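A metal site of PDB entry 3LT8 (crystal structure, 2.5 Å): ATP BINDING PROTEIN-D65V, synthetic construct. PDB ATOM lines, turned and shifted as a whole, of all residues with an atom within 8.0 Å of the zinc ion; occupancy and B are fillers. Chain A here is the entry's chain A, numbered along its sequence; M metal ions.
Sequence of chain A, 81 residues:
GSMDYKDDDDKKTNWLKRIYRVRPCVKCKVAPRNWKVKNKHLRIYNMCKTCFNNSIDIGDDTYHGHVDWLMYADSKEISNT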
ATOM      1  N   PRO A  24      15.160 -23.570 -30.490  1.00  0.00           N
ATOM      2  CA  PRO A  24      14.416 -22.366 -30.886  1.00  0.00           C
ATOM      3  C   PRO A  24      13.163 -22.188 -30.016  1.00  0.00           C
ATOM      4  O   PRO A  24      12.876 -23.053 -29.179  1.00  0.00           O
ATOM      5  CB  PRO A  24      13.987 -22.671 -32.322  1.00  0.00           C
ATOM      6  CG  PRO A  24      13.967 -24.174 -32.398  1.00  0.00           C
ATOM      7  CD  PRO A  24      15.035 -24.661 -31.476  1.00  0.00           C
ATOM      8  N   CYS A  25      12.454 -21.076 -30.212  1.00  0.00           N
ATOM      9  CA  CYS A  25      11.173 -20.790 -29.580  1.00  0.00           C
ATOM     10  C   CYS A  25      10.307 -22.041 -29.316  1.00  0.00           C
ATOM     11  O   CYS A  25      10.084 -22.812 -30.248  1.00  0.00           O
ATOM     12  CB  CYS A  25      10.405 -19.862 -30.516  1.00  0.00           C
ATOM     13  SG  CYS A  25       8.813 -19.369 -29.880  1.00  0.00           S
ATOM     14  N   VAL A  26       9.810 -22.249 -28.097  1.00  0.00           N
ATOM     15  CA  VAL A  26       8.981 -23.440 -27.865  1.00  0.00           C
ATOM     16  C   VAL A  26       7.660 -23.375 -28.650  1.00  0.00           C
ATOM     17  O   VAL A  26       7.004 -24.394 -28.853  1.00  0.00           O
ATOM     18  CB  VAL A  26       8.616 -23.671 -26.360  1.00  0.00           C
ATOM     19  CG1 VAL A  26       9.823 -24.089 -25.528  1.00  0.00           C
ATOM     20  CG2 VAL A  26       7.935 -22.456 -25.780  1.00  0.00           C
ATOM     21  N   LYS A  27       7.248 -22.184 -29.068  1.00  0.00           N
ATOM     22  CA  LYS A  27       5.915 -22.036 -29.617  1.00  0.00           C
ATOM     23  C   LYS A  27       5.887 -22.131 -31.126  1.00  0.00           C
ATOM     24  O   LYS A  27       5.135 -22.941 -31.674  1.00  0.00           O
ATOM     25  CB  LYS A  27       5.234 -20.757 -29.133  1.00  0.00           C
ATOM     26  CG  LYS A  27       3.865 -20.527 -29.727  1.00  0.00           C
ATOM     27  CD  LYS A  27       2.933 -21.683 -29.432  1.00  0.00           C
ATOM     28  CE  LYS A  27       1.610 -21.491 -30.148  1.00  0.00           C
ATOM     29  NZ  LYS A  27       0.641 -22.551 -29.749  1.00  0.00           N
ATOM     30  N   CYS A  28       6.681 -21.314 -31.803  1.00  0.00           N
ATOM     31  CA  CYS A  28       6.747 -21.400 -33.270  1.00  0.00           C
ATOM     32  C   CYS A  28       7.810 -22.373 -33.736  1.00  0.00           C
ATOM     33  O   CYS A  28       7.804 -22.768 -34.881  1.00  0.00           O
ATOM     34  CB  CYS A  28       7.003 -20.033 -33.901  1.00  0.00           C
ATOM     35  SG  CYS A  28       8.696 -19.408 -33.571  1.00  0.00           S
ATOM     36  N   LYS A  29       8.745 -22.745 -32.858  1.00  0.00           N
ATOM     37  CA  LYS A  29       9.729 -23.767 -33.225  1.00  0.00           C
ATOM     38  C   LYS A  29      10.812 -23.367 -34.224  1.00  0.00           C
ATOM     39  O   LYS A  29      11.719 -24.146 -34.420  1.00  0.00           O
ATOM     40  CB  LYS A  29       9.030 -24.967 -33.839  1.00  0.00           C
ATOM     41  CG  LYS A  29       7.763 -25.348 -33.171  1.00  0.00           C
ATOM     42  CD  LYS A  29       8.035 -26.199 -32.009  1.00  0.00           C
ATOM     43  CE  LYS A  29       6.728 -26.680 -31.416  1.00  0.00           C
ATOM     44  NZ  LYS A  29       7.092 -27.479 -30.208  1.00  0.00           N
ATOM     45  N   VAL A  30      10.707 -22.210 -34.883  1.00  0.00           N
ATOM     46  CA  VAL A  30      11.778 -21.741 -35.795  1.00  0.00           C
ATOM     47  C   VAL A  30      12.592 -20.549 -35.252  1.00  0.00           C
ATOM     48  O   VAL A  30      13.822 -20.617 -35.152  1.00  0.00           O
ATOM     49  CB  VAL A  30      11.235 -21.364 -37.177  1.00  0.00           C
ATOM     50  CG1 VAL A  30      12.391 -21.296 -38.173  1.00  0.00           C
ATOM     51  CG2 VAL A  30      10.229 -22.399 -37.645  1.00  0.00           C
ATOM     52  N   ALA A  31      11.945 -19.430 -34.923  1.00  0.00           N
ATOM     53  CA  ALA A  31      12.683 -18.328 -34.363  1.00  0.00           C
ATOM     54  C   ALA A  31      13.478 -18.710 -33.105  1.00  0.00           C
ATOM     55  O   ALA A  31      13.110 -19.600 -32.321  1.00  0.00           O
ATOM     56  CB  ALA A  31      11.780 -17.173 -34.068  1.00  0.00           C
ATOM     57  N   PRO A  32      14.609 -18.048 -32.913  1.00  0.00           N
ATOM     58  CA  PRO A  32      15.338 -18.241 -31.679  1.00  0.00           C
ATOM     59  C   PRO A  32      14.649 -17.498 -30.550  1.00  0.00           C
ATOM     60  O   PRO A  32      13.801 -16.629 -30.789  1.00  0.00           O
ATOM     61  CB  PRO A  32      16.711 -17.645 -31.987  1.00  0.00           C
ATOM     62  CG  PRO A  32      16.465 -16.687 -33.127  1.00  0.00           C
ATOM     63  CD  PRO A  32      15.357 -17.273 -33.916  1.00  0.00           C
ATOM     64  N   ARG A  33      14.979 -17.863 -29.320  1.00  0.00           N
ATOM     65  CA  ARG A  33      14.256 -17.322 -28.155  1.00  0.00           C
ATOM     66  C   ARG A  33      14.639 -15.875 -27.811  1.00  0.00           C
ATOM     67  O   ARG A  33      15.768 -15.407 -28.096  1.00  0.00           O
ATOM     68  CB  ARG A  33      14.491 -18.217 -26.936  1.00  0.00           C
ATOM     69  CG  ARG A  33      13.759 -19.512 -27.012  1.00  0.00           C
ATOM     70  CD  ARG A  33      14.351 -20.495 -26.033  1.00  0.00           C
ATOM     71  NE  ARG A  33      13.950 -21.843 -26.410  1.00  0.00           N
ATOM     72  CZ  ARG A  33      13.738 -22.816 -25.534  1.00  0.00           C
ATOM     73  NH1 ARG A  33      13.897 -22.577 -24.230  1.00  0.00           N
ATOM     74  NH2 ARG A  33      13.364 -24.013 -25.959  1.00  0.00           N
ATOM     75  N   ASN A  34      13.703 -15.158 -27.200  1.00  0.00           N
ATOM     76  CA  ASN A  34      14.091 -13.916 -26.573  1.00  0.00           C
ATOM     77  C   ASN A  34      15.045 -14.187 -25.399  1.00  0.00           C
ATOM     78  O   ASN A  34      15.091 -15.308 -24.889  1.00  0.00           O
ATOM     79  CB  ASN A  34      12.892 -13.122 -26.100  1.00  0.00           C
ATOM     80  CG  ASN A  34      13.208 -11.646 -25.948  1.00  0.00           C
ATOM     81  OD1 ASN A  34      14.259 -11.158 -26.393  1.00  0.00           O
ATOM     82  ND2 ASN A  34      12.304 -10.922 -25.330  1.00  0.00           N
ATOM     83  N   ASN A  46      11.385 -18.694 -22.873  1.00  0.00           N
ATOM     84  CA  ASN A  46      10.964 -19.847 -23.650  1.00  0.00           C
ATOM     85  C   ASN A  46      10.540 -19.529 -25.103  1.00  0.00           C
ATOM     86  O   ASN A  46      10.590 -20.403 -25.978  1.00  0.00           O
ATOM     87  CB  ASN A  46       9.849 -20.620 -22.912  1.00  0.00           C
ATOM     88  CG  ASN A  46      10.238 -20.999 -21.501  1.00  0.00           C
ATOM     89  OD1 ASN A  46      11.436 -21.203 -21.180  1.00  0.00           O
ATOM     90  ND2 ASN A  46       9.240 -21.119 -20.631  1.00  0.00           N
ATOM     91  N   MET A  47      10.118 -18.283 -25.363  1.00  0.00           N
ATOM     92  CA  MET A  47       9.612 -17.920 -26.699  1.00  0.00           C
ATOM     93  C   MET A  47      10.330 -16.735 -27.344  1.00  0.00           C
ATOM     94  O   MET A  47      10.960 -15.929 -26.642  1.00  0.00           O
ATOM     95  CB  MET A  47       8.140 -17.588 -26.614  1.00  0.00           C
ATOM     96  CG  MET A  47       7.226 -18.768 -26.363  1.00  0.00           C
ATOM     97  SD  MET A  47       5.472 -18.259 -26.412  1.00  0.00           S
ATOM     98  CE  MET A  47       5.346 -17.303 -24.868  1.00  0.00           C
ATOM     99  N   CYS A  48      10.227 -16.612 -28.662  1.00  0.00           N
ATOM    100  CA  CYS A  48      10.763 -15.399 -29.311  1.00  0.00           C
ATOM    101  C   CYS A  48       9.831 -14.274 -28.908  1.00  0.00           C
ATOM    102  O   CYS A  48       8.820 -14.537 -28.231  1.00  0.00           O
ATOM    103  CB  CYS A  48      10.807 -15.556 -30.826  1.00  0.00           C
ATOM    104  SG  CYS A  48       9.175 -15.775 -31.574  1.00  0.00           S
ATOM    105  N   LYS A  49      10.148 -13.040 -29.285  1.00  0.00           N
ATOM    106  CA  LYS A  49       9.316 -11.922 -28.829  1.00  0.00           C
ATOM    107  C   LYS A  49       7.960 -11.920 -29.531  1.00  0.00           C
ATOM    108  O   LYS A  49       6.934 -11.589 -28.900  1.00  0.00           O
ATOM    109  CB  LYS A  49      10.017 -10.588 -29.051  1.00  0.00           C
ATOM    110  CG  LYS A  49       9.213  -9.336 -28.705  1.00  0.00           C
ATOM    111  CD  LYS A  49       9.689  -8.762 -27.389  1.00  0.00           C
ATOM    112  CE  LYS A  49       8.925  -7.500 -27.001  1.00  0.00           C
ATOM    113  NZ  LYS A  49       8.988  -6.469 -28.102  1.00  0.00           N
ATOM    114  N   THR A  50       7.952 -12.286 -30.821  1.00  0.00           N
ATOM    115  CA  THR A  50       6.729 -12.281 -31.590  1.00  0.00           C
ATOM    116  C   THR A  50       5.686 -13.216 -30.982  1.00  0.00           C
ATOM    117  O   THR A  50       4.516 -12.833 -30.829  1.00  0.00           O
ATOM    118  CB  THR A  50       6.967 -12.679 -33.058  1.00  0.00           C
ATOM    119  OG1 THR A  50       7.970 -11.846 -33.652  1.00  0.00           O
ATOM    120  CG2 THR A  50       5.652 -12.536 -33.849  1.00  0.00           C
ATOM    121  N   CYS A  51       6.103 -14.427 -30.612  1.00  0.00           N
ATOM    122  CA  CYS A  51       5.183 -15.411 -30.047  1.00  0.00           C
ATOM    123  C   CYS A  51       4.832 -15.088 -28.608  1.00  0.00           C
ATOM    124  O   CYS A  51       3.733 -15.387 -28.162  1.00  0.00           O
ATOM    125  CB  CYS A  51       5.739 -16.852 -30.153  1.00  0.00           C
ATOM    126  SG  CYS A  51       5.918 -17.492 -31.865  1.00  0.00           S
ATOM    127  N   PHE A  52       5.746 -14.470 -27.863  1.00  0.00           N
ATOM    128  CA  PHE A  52       5.356 -14.058 -26.514  1.00  0.00           C
ATOM    129  C   PHE A  52       4.232 -13.000 -26.538  1.00  0.00           C
ATOM    130  O   PHE A  52       3.211 -13.156 -25.852  1.00  0.00           O
ATOM    131  CB  PHE A  52       6.542 -13.554 -25.728  1.00  0.00           C
ATOM    132  CG  PHE A  52       6.175 -13.060 -24.352  1.00  0.00           C
ATOM    133  CD1 PHE A  52       5.729 -13.934 -23.381  1.00  0.00           C
ATOM    134  CD2 PHE A  52       6.275 -11.689 -24.034  1.00  0.00           C
ATOM    135  CE1 PHE A  52       5.385 -13.481 -22.099  1.00  0.00           C
ATOM    136  CE2 PHE A  52       5.936 -11.232 -22.767  1.00  0.00           C
ATOM    137  CZ  PHE A  52       5.488 -12.130 -21.791  1.00  0.00           C
HETATM  138 ZN    ZN M   1       8.214 -18.113 -31.770  1.00  0.00          ZN
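N of Ala 31 lies close to SG of Cys 28 (3.5 Å). N of Val 30 sits close to SG of Cys 28, at 3.7 Å. The backbone NH of Cys 25 is in hydrogen-bond range of the backbone carbonyl oxygen of Ala 31, 2.7 Å away. SG of Cys 25 sits close to N of Lys 27. N of Thr 50 lies close to SG of Cys 48.
SG of Cys 28 is bound to the zinc ion (2.3 Å). SG of Cys 25 is bound to the zinc ion (2.3 Å). The zinc ion is bound by the side-chain sulfur (SG) of Cys 51. SG of Cys 48 binds the zinc ion (2.5 Å).
Of the 18 residues printed, 4 come within 4 Å of the zinc ion. Along chain A the residues within 4 Å of the zinc ion span positions 25 to 51.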
